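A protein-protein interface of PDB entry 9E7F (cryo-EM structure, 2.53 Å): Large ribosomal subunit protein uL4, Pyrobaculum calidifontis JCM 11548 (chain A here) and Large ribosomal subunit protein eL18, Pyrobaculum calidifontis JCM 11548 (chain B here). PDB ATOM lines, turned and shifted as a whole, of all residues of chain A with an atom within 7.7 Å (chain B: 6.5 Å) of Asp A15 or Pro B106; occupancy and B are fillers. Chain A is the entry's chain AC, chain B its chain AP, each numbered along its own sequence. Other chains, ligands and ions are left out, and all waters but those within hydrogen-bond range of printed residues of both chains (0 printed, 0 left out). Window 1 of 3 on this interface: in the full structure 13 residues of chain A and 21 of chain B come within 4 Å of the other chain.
The backbone NH (N) of Ala B84 lies within hydrogen-bond range of the backbone carbonyl oxygen (O) of Leu B103. N of Glu B107 sits close to OG1 of Thr B104, 3.1 Å away. The side-chain carboxylate (OD1) of Asp A15 is in hydrogen-bond range of the side-chain hydroxyl (OG) of Ser A17 (2.6 Å).
Of the 13 printed residues of chain B, 7 touch a printed residue of chain A. Printed residues of chain B that touch a printed residue of chain A: Phe B19, Ala B84, Leu B103, Thr B104, Pro B106, Glu B107 and Arg B110. Of the 13 printed residues of chain A, 7 touch a printed residue of chain B. Printed residues of chain A that touch a printed residue of chain B: Lys A10, Phe A11, Asp A15, Leu A16, Ser A17, Tyr A19 and Ile A20. Hydrophobic or aromatic side chains of chain A within 4 Å of the printed part of chain B: Phe A11, Leu A16, Tyr A19 and Ile A20.
Among the printed residues, merely in contact across the chains: Lys A10 with Leu B103 (3.99 Å), Lys A10 with Thr B104 (3.8 Å), Phe A11 with Ala B84 (3.1 Å), Phe A11 with Leu B103 (3.6 Å), Asp A15 with Pro B106 (3.2 Å), Leu A16 with Phe B19 (3.1 Å), Ser A17 with Phe B19 (3.7 Å), Tyr A19 with Phe B19 (3.4 Å) and Ile A20 with Phe B19 (3.9 Å).
The side-chain carboxylate (OE1) of Glu B107 is in salt-bridge range of the side-chain amino group (NZ) of Lys A10 (3.7 Å). The guanidinium group of Arg B110 is in salt-bridge range of the side-chain carboxylate of Asp A15 (3.6 Å). NH1 of Arg B110 is in hydrogen-bond range of O of Ser A17.
Leu A9 touches none of the printed residues of chain B. Of the printed residues of chain B, Lys A10 touches Leu B103 (3.99 Å), Thr B104 (3.8 Å) and Glu B107 (3.5 Å). Of chain B, only Pro B106 and Arg B110 come within 4 Å of Asp A15. Printed residues of chain A within 4 Å of Phe B19: Leu A16 (3.1 Å), Ser A17 (3.7 Å), Tyr A19 (3.4 Å) and Ile A20 (3.9 Å). Pro B106 touches one residue of chain A. Leu B108 touches none of the printed residues of chain A. The nearest printed residue of chain B that does not touch Asp A15 is Phe B19 (5.3 Å). The nearest residue of chain A that does not touch Pro B106 is Leu A14 (4.02 Å).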
ATOM      1  N   LEU A   9     -22.925 -26.628 -15.430  1.00  0.00           N
ATOM      2  CA  LEU A   9     -23.284 -25.704 -16.493  1.00  0.00           C
ATOM      3  C   LEU A   9     -23.649 -24.320 -15.963  1.00  0.00           C
ATOM      4  O   LEU A   9     -24.346 -23.567 -16.650  1.00  0.00           O
ATOM      5  CB  LEU A   9     -24.440 -26.277 -17.313  1.00  0.00           C
ATOM      6  CG  LEU A   9     -24.353 -27.760 -17.688  1.00  0.00           C
ATOM      7  CD1 LEU A   9     -25.112 -28.624 -16.697  1.00  0.00           C
ATOM      8  CD2 LEU A   9     -24.883 -27.981 -19.094  1.00  0.00           C
ATOM      9  N   LYS A  10     -23.192 -23.976 -14.756  1.00  0.00           N
ATOM     10  CA  LYS A  10     -23.594 -22.716 -14.139  1.00  0.00           C
ATOM     11  C   LYS A  10     -23.041 -21.517 -14.897  1.00  0.00           C
ATOM     12  O   LYS A  10     -23.708 -20.483 -15.006  1.00  0.00           O
ATOM     13  CB  LYS A  10     -23.154 -22.687 -12.675  1.00  0.00           C
ATOM     14  CG  LYS A  10     -21.658 -22.790 -12.469  1.00  0.00           C
ATOM     15  CD  LYS A  10     -21.325 -23.363 -11.107  1.00  0.00           C
ATOM     16  CE  LYS A  10     -21.043 -22.256 -10.114  1.00  0.00           C
ATOM     17  NZ  LYS A  10     -20.500 -22.759  -8.830  1.00  0.00           N
ATOM     18  N   PHE A  11     -21.823 -21.628 -15.424  1.00  0.00           N
ATOM     19  CA  PHE A  11     -21.295 -20.568 -16.273  1.00  0.00           C
ATOM     20  C   PHE A  11     -21.930 -20.581 -17.655  1.00  0.00           C
ATOM     21  O   PHE A  11     -21.932 -19.549 -18.331  1.00  0.00           O
ATOM     22  CB  PHE A  11     -19.780 -20.694 -16.407  1.00  0.00           C
ATOM     23  CG  PHE A  11     -19.029 -20.312 -15.170  1.00  0.00           C
ATOM     24  CD1 PHE A  11     -18.814 -21.234 -14.165  1.00  0.00           C
ATOM     25  CD2 PHE A  11     -18.529 -19.037 -15.018  1.00  0.00           C
ATOM     26  CE1 PHE A  11     -18.125 -20.888 -13.031  1.00  0.00           C
ATOM     27  CE2 PHE A  11     -17.833 -18.684 -13.882  1.00  0.00           C
ATOM     28  CZ  PHE A  11     -17.632 -19.610 -12.889  1.00  0.00           C
ATOM     29  N   LYS A  12     -22.471 -21.722 -18.084  1.00  0.00           N
ATOM     30  CA  LYS A  12     -23.076 -21.804 -19.409  1.00  0.00           C
ATOM     31  C   LYS A  12     -24.393 -21.044 -19.455  1.00  0.00           C
ATOM     32  O   LYS A  12     -24.515 -20.026 -20.145  1.00  0.00           O
ATOM     33  CB  LYS A  12     -23.295 -23.267 -19.793  1.00  0.00           C
ATOM     34  CG  LYS A  12     -23.537 -23.488 -21.270  1.00  0.00           C
ATOM     35  CD  LYS A  12     -23.084 -24.862 -21.691  1.00  0.00           C
ATOM     36  CE  LYS A  12     -21.731 -25.184 -21.114  1.00  0.00           C
ATOM     37  NZ  LYS A  12     -20.646 -24.737 -22.018  1.00  0.00           N
ATOM     38  N   LEU A  13     -25.386 -21.512 -18.707  1.00  0.00           N
ATOM     39  CA  LEU A  13     -26.667 -20.821 -18.613  1.00  0.00           C
ATOM     40  C   LEU A  13     -26.576 -19.899 -17.410  1.00  0.00           C
ATOM     41  O   LEU A  13     -26.891 -20.275 -16.283  1.00  0.00           O
ATOM     42  CB  LEU A  13     -27.821 -21.806 -18.493  1.00  0.00           C
ATOM     43  CG  LEU A  13     -29.070 -21.399 -19.280  1.00  0.00           C
ATOM     44  CD1 LEU A  13     -28.986 -21.898 -20.716  1.00  0.00           C
ATOM     45  CD2 LEU A  13     -30.338 -21.885 -18.606  1.00  0.00           C
ATOM     46  N   LEU A  14     -26.124 -18.675 -17.658  1.00  0.00           N
ATOM     47  CA  LEU A  14     -25.888 -17.731 -16.579  1.00  0.00           C
ATOM     48  C   LEU A  14     -27.211 -17.235 -16.013  1.00  0.00           C
ATOM     49  O   LEU A  14     -28.081 -16.767 -16.753  1.00  0.00           O
ATOM     50  CB  LEU A  14     -25.052 -16.562 -17.091  1.00  0.00           C
ATOM     51  CG  LEU A  14     -24.328 -15.718 -16.052  1.00  0.00           C
ATOM     52  CD1 LEU A  14     -23.304 -16.557 -15.324  1.00  0.00           C
ATOM     53  CD2 LEU A  14     -23.663 -14.534 -16.724  1.00  0.00           C
ATOM     54  N   ASP A  15     -27.362 -17.337 -14.696  1.00  0.00           N
ATOM     55  CA  ASP A  15     -28.563 -16.886 -14.009  1.00  0.00           C
ATOM     56  C   ASP A  15     -28.359 -15.413 -13.673  1.00  0.00           C
ATOM     57  O   ASP A  15     -27.452 -15.065 -12.912  1.00  0.00           O
ATOM     58  CB  ASP A  15     -28.803 -17.735 -12.757  1.00  0.00           C
ATOM     59  CG  ASP A  15     -30.112 -17.405 -12.022  1.00  0.00           C
ATOM     60  OD1 ASP A  15     -30.752 -16.358 -12.256  1.00  0.00           O
ATOM     61  OD2 ASP A  15     -30.505 -18.227 -11.171  1.00  0.00           O
ATOM     62  N   LEU A  16     -29.202 -14.555 -14.237  1.00  0.00           N
ATOM     63  CA  LEU A  16     -29.040 -13.114 -14.116  1.00  0.00           C
ATOM     64  C   LEU A  16     -30.101 -12.473 -13.233  1.00  0.00           C
ATOM     65  O   LEU A  16     -30.207 -11.245 -13.206  1.00  0.00           O
ATOM     66  CB  LEU A  16     -29.045 -12.466 -15.499  1.00  0.00           C
ATOM     67  CG  LEU A  16     -27.708 -12.451 -16.245  1.00  0.00           C
ATOM     68  CD1 LEU A  16     -26.651 -11.711 -15.429  1.00  0.00           C
ATOM     69  CD2 LEU A  16     -27.236 -13.851 -16.596  1.00  0.00           C
ATOM     70  N   SER A  17     -30.889 -13.267 -12.518  1.00  0.00           N
ATOM     71  CA  SER A  17     -31.854 -12.713 -11.590  1.00  0.00           C
ATOM     72  C   SER A  17     -31.147 -12.201 -10.339  1.00  0.00           C
ATOM     73  O   SER A  17     -30.053 -12.656 -10.002  1.00  0.00           O
ATOM     74  CB  SER A  17     -32.885 -13.766 -11.210  1.00  0.00           C
ATOM     75  OG  SER A  17     -32.248 -14.935 -10.732  1.00  0.00           O
ATOM     76  N   PRO A  18     -31.766 -11.263  -9.617  1.00  0.00           N
ATOM     77  CA  PRO A  18     -33.069 -10.644  -9.867  1.00  0.00           C
ATOM     78  C   PRO A  18     -32.997  -9.321 -10.624  1.00  0.00           C
ATOM     79  O   PRO A  18     -34.032  -8.755 -10.958  1.00  0.00           O
ATOM     80  CB  PRO A  18     -33.601 -10.439  -8.450  1.00  0.00           C
ATOM     81  CG  PRO A  18     -32.361 -10.085  -7.665  1.00  0.00           C
ATOM     82  CD  PRO A  18     -31.214 -10.833  -8.320  1.00  0.00           C
ATOM     83  N   TYR A  19     -31.806  -8.798 -10.911  1.00  0.00           N
ATOM     84  CA  TYR A  19     -31.694  -7.497 -11.559  1.00  0.00           C
ATOM     85  C   TYR A  19     -31.928  -7.549 -13.063  1.00  0.00           C
ATOM     86  O   TYR A  19     -32.020  -6.490 -13.692  1.00  0.00           O
ATOM     87  CB  TYR A  19     -30.328  -6.880 -11.264  1.00  0.00           C
ATOM     88  CG  TYR A  19     -30.007  -6.809  -9.789  1.00  0.00           C
ATOM     89  CD1 TYR A  19     -30.627  -5.882  -8.968  1.00  0.00           C
ATOM     90  CD2 TYR A  19     -29.091  -7.674  -9.216  1.00  0.00           C
ATOM     91  CE1 TYR A  19     -30.339  -5.819  -7.625  1.00  0.00           C
ATOM     92  CE2 TYR A  19     -28.799  -7.620  -7.877  1.00  0.00           C
ATOM     93  CZ  TYR A  19     -29.423  -6.692  -7.084  1.00  0.00           C
ATOM     94  OH  TYR A  19     -29.126  -6.637  -5.742  1.00  0.00           O
ATOM     95  N   ILE A  20     -32.013  -8.737 -13.655  1.00  0.00           N
ATOM     96  CA  ILE A  20     -32.419  -8.905 -15.045  1.00  0.00           C
ATOM     97  C   ILE A  20     -33.495  -9.976 -15.078  1.00  0.00           C
ATOM     98  O   ILE A  20     -33.319 -11.048 -14.492  1.00  0.00           O
ATOM     99  CB  ILE A  20     -31.242  -9.302 -15.957  1.00  0.00           C
ATOM    100  CG1 ILE A  20     -29.998  -8.463 -15.653  1.00  0.00           C
ATOM    101  CG2 ILE A  20     -31.625  -9.144 -17.411  1.00  0.00           C
ATOM    102  CD1 ILE A  20     -30.123  -7.007 -16.019  1.00  0.00           C
ATOM    103  N   PRO A  22     -35.545 -13.081 -16.308  1.00  0.00           N
ATOM    104  CA  PRO A  22     -35.166 -14.230 -17.134  1.00  0.00           C
ATOM    105  C   PRO A  22     -35.962 -14.287 -18.429  1.00  0.00           C
ATOM    106  O   PRO A  22     -37.089 -13.796 -18.521  1.00  0.00           O
ATOM    107  CB  PRO A  22     -35.482 -15.433 -16.237  1.00  0.00           C
ATOM    108  CG  PRO A  22     -35.602 -14.865 -14.850  1.00  0.00           C
ATOM    109  CD  PRO A  22     -36.152 -13.494 -15.034  1.00  0.00           C
ATOM    110  N   LEU B  16     -24.086  -9.480 -18.336  1.00  0.00           N
ATOM    111  CA  LEU B  16     -23.407  -9.478 -17.045  1.00  0.00           C
ATOM    112  C   LEU B  16     -22.909  -8.083 -16.688  1.00  0.00           C
ATOM    113  O   LEU B  16     -22.943  -7.684 -15.520  1.00  0.00           O
ATOM    114  CB  LEU B  16     -22.258 -10.484 -17.058  1.00  0.00           C
ATOM    115  CG  LEU B  16     -21.310 -10.461 -15.858  1.00  0.00           C
ATOM    116  CD1 LEU B  16     -22.071 -10.562 -14.549  1.00  0.00           C
ATOM    117  CD2 LEU B  16     -20.291 -11.576 -15.973  1.00  0.00           C
ATOM    118  N   PHE B  19     -25.887  -6.374 -15.614  1.00  0.00           N
ATOM    119  CA  PHE B  19     -26.299  -6.894 -14.315  1.00  0.00           C
ATOM    120  C   PHE B  19     -25.537  -6.222 -13.185  1.00  0.00           C
ATOM    121  O   PHE B  19     -26.121  -5.857 -12.160  1.00  0.00           O
ATOM    122  CB  PHE B  19     -26.090  -8.412 -14.280  1.00  0.00           C
ATOM    123  CG  PHE B  19     -26.399  -9.049 -12.950  1.00  0.00           C
ATOM    124  CD1 PHE B  19     -25.394  -9.311 -12.027  1.00  0.00           C
ATOM    125  CD2 PHE B  19     -27.693  -9.409 -12.632  1.00  0.00           C
ATOM    126  CE1 PHE B  19     -25.682  -9.884 -10.817  1.00  0.00           C
ATOM    127  CE2 PHE B  19     -27.979  -9.995 -11.428  1.00  0.00           C
ATOM    128  CZ  PHE B  19     -26.974 -10.229 -10.516  1.00  0.00           C
ATOM    129  N   LEU B  20     -24.221  -6.079 -13.343  1.00  0.00           N
ATOM    130  CA  LEU B  20     -23.399  -5.558 -12.258  1.00  0.00           C
ATOM    131  C   LEU B  20     -23.708  -4.097 -11.978  1.00  0.00           C
ATOM    132  O   LEU B  20     -23.707  -3.671 -10.819  1.00  0.00           O
ATOM    133  CB  LEU B  20     -21.921  -5.736 -12.583  1.00  0.00           C
ATOM    134  CG  LEU B  20     -21.362  -7.134 -12.357  1.00  0.00           C
ATOM    135  CD1 LEU B  20     -19.971  -7.239 -12.930  1.00  0.00           C
ATOM    136  CD2 LEU B  20     -21.366  -7.480 -10.890  1.00  0.00           C
ATOM    137  N   ALA B  84     -15.622 -15.873 -10.793  1.00  0.00           N
ATOM    138  CA  ALA B  84     -14.926 -15.456 -11.998  1.00  0.00           C
ATOM    139  C   ALA B  84     -15.919 -15.270 -13.131  1.00  0.00           C
ATOM    140  O   ALA B  84     -17.047 -15.761 -13.084  1.00  0.00           O
ATOM    141  CB  ALA B  84     -13.846 -16.463 -12.402  1.00  0.00           C
ATOM    142  N   LEU B 103     -17.578 -19.861  -7.893  1.00  0.00           N
ATOM    143  CA  LEU B 103     -18.868 -19.206  -8.020  1.00  0.00           C
ATOM    144  C   LEU B 103     -18.920 -18.395  -9.302  1.00  0.00           C
ATOM    145  O   LEU B 103     -17.898 -17.900  -9.780  1.00  0.00           O
ATOM    146  CB  LEU B 103     -19.130 -18.270  -6.845  1.00  0.00           C
ATOM    147  CG  LEU B 103     -19.953 -18.796  -5.685  1.00  0.00           C
ATOM    148  CD1 LEU B 103     -19.395 -20.117  -5.268  1.00  0.00           C
ATOM    149  CD2 LEU B 103     -19.906 -17.810  -4.543  1.00  0.00           C
ATOM    150  N   THR B 104     -20.117 -18.259  -9.856  1.00  0.00           N
ATOM    151  CA  THR B 104     -20.332 -17.238 -10.866  1.00  0.00           C
ATOM    152  C   THR B 104     -20.434 -15.880 -10.185  1.00  0.00           C
ATOM    153  O   THR B 104     -20.759 -15.780  -9.000  1.00  0.00           O
ATOM    154  CB  THR B 104     -21.592 -17.518 -11.684  1.00  0.00           C
ATOM    155  OG1 THR B 104     -22.752 -17.302 -10.876  1.00  0.00           O
ATOM    156  CG2 THR B 104     -21.596 -18.945 -12.195  1.00  0.00           C
ATOM    157  N   ILE B 105     -20.117 -14.832 -10.940  1.00  0.00           N
ATOM    158  CA  ILE B 105     -20.255 -13.472 -10.413  1.00  0.00           C
ATOM    159  C   ILE B 105     -21.691 -13.125 -10.030  1.00  0.00           C
ATOM    160  O   ILE B 105     -21.885 -12.497  -8.977  1.00  0.00           O
ATOM    161  CB  ILE B 105     -19.647 -12.460 -11.399  1.00  0.00           C
ATOM    162  CG1 ILE B 105     -18.129 -12.415 -11.230  1.00  0.00           C
ATOM    163  CG2 ILE B 105     -20.246 -11.089 -11.170  1.00  0.00           C
ATOM    164  CD1 ILE B 105     -17.453 -11.288 -11.980  1.00  0.00           C
ATOM    165  N   PRO B 106     -22.722 -13.436 -10.836  1.00  0.00           N
ATOM    166  CA  PRO B 106     -24.096 -13.183 -10.368  1.00  0.00           C
ATOM    167  C   PRO B 106     -24.456 -13.954  -9.116  1.00  0.00           C
ATOM    168  O   PRO B 106     -25.242 -13.465  -8.297  1.00  0.00           O
ATOM    169  CB  PRO B 106     -24.956 -13.623 -11.558  1.00  0.00           C
ATOM    170  CG  PRO B 106     -24.088 -13.485 -12.717  1.00  0.00           C
ATOM    171  CD  PRO B 106     -22.719 -13.834 -12.257  1.00  0.00           C
ATOM    172  N   GLU B 107     -23.897 -15.146  -8.947  1.00  0.00           N
ATOM    173  CA  GLU B 107     -24.151 -15.935  -7.751  1.00  0.00           C
ATOM    174  C   GLU B 107     -23.550 -15.280  -6.513  1.00  0.00           C
ATOM    175  O   GLU B 107     -24.148 -15.315  -5.434  1.00  0.00           O
ATOM    176  CB  GLU B 107     -23.601 -17.341  -7.963  1.00  0.00           C
ATOM    177  CG  GLU B 107     -23.769 -18.287  -6.817  1.00  0.00           C
ATOM    178  CD  GLU B 107     -23.322 -19.678  -7.190  1.00  0.00           C
ATOM    179  OE1 GLU B 107     -22.724 -19.832  -8.275  1.00  0.00           O
ATOM    180  OE2 GLU B 107     -23.566 -20.617  -6.404  1.00  0.00           O
ATOM    181  N   LEU B 108     -22.367 -14.678  -6.649  1.00  0.00           N
ATOM    182  CA  LEU B 108     -21.746 -14.007  -5.512  1.00  0.00           C
ATOM    183  C   LEU B 108     -22.539 -12.780  -5.083  1.00  0.00           C
ATOM    184  O   LEU B 108     -22.639 -12.487  -3.886  1.00  0.00           O
ATOM    185  CB  LEU B 108     -20.312 -13.611  -5.847  1.00  0.00           C
ATOM    186  CG  LEU B 108     -19.596 -12.958  -4.670  1.00  0.00           C
ATOM    187  CD1 LEU B 108     -19.810 -13.782  -3.417  1.00  0.00           C
ATOM    188  CD2 LEU B 108     -18.121 -12.779  -4.956  1.00  0.00           C
ATOM    189  N   VAL B 109     -23.089 -12.037  -6.045  1.00  0.00           N
ATOM    190  CA  VAL B 109     -23.905 -10.873  -5.715  1.00  0.00           C
ATOM    191  C   VAL B 109     -25.177 -11.300  -4.997  1.00  0.00           C
ATOM    192  O   VAL B 109     -25.613 -10.653  -4.038  1.00  0.00           O
ATOM    193  CB  VAL B 109     -24.215 -10.060  -6.984  1.00  0.00           C
ATOM    194  CG1 VAL B 109     -25.171  -8.926  -6.668  1.00  0.00           C
ATOM    195  CG2 VAL B 109     -22.937  -9.525  -7.590  1.00  0.00           C
ATOM    196  N   ARG B 110     -25.797 -12.390  -5.456  1.00  0.00           N
ATOM    197  CA  ARG B 110     -26.984 -12.911  -4.785  1.00  0.00           C
ATOM    198  C   ARG B 110     -26.654 -13.402  -3.382  1.00  0.00           C
ATOM    199  O   ARG B 110     -27.431 -13.196  -2.445  1.00  0.00           O
ATOM    200  CB  ARG B 110     -27.602 -14.039  -5.606  1.00  0.00           C
ATOM    201  CG  ARG B 110     -28.210 -13.603  -6.917  1.00  0.00           C
ATOM    202  CD  ARG B 110     -29.170 -14.653  -7.431  1.00  0.00           C
ATOM    203  NE  ARG B 110     -28.473 -15.846  -7.894  1.00  0.00           N
ATOM    204  CZ  ARG B 110     -28.011 -16.011  -9.125  1.00  0.00           C
ATOM    205  NH1 ARG B 110     -28.156 -15.076 -10.048  1.00  0.00           N
ATOM    206  NH2 ARG B 110     -27.391 -17.145  -9.439  1.00  0.00           N
ATOM    207  N   ARG B 111     -25.512 -14.065  -3.222  1.00  0.00           N
ATOM    208  CA  ARG B 111     -25.107 -14.523  -1.899  1.00  0.00           C
ATOM    209  C   ARG B 111     -24.645 -13.364  -1.024  1.00  0.00           C
ATOM    210  O   ARG B 111     -24.920 -13.341   0.180  1.00  0.00           O
ATOM    211  CB  ARG B 111     -24.007 -15.573  -2.030  1.00  0.00           C
ATOM    212  CG  ARG B 111     -23.268 -15.856  -0.749  1.00  0.00           C
ATOM    213  CD  ARG B 111     -22.099 -16.784  -1.002  1.00  0.00           C
ATOM    214  NE  ARG B 111     -22.513 -17.985  -1.715  1.00  0.00           N
ATOM    215  CZ  ARG B 111     -21.759 -19.065  -1.856  1.00  0.00           C
ATOM    216  NH1 ARG B 111     -20.548 -19.136  -1.332  1.00  0.00           N
ATOM    217  NH2 ARG B 111     -22.235 -20.103  -2.535  1.00  0.00           N
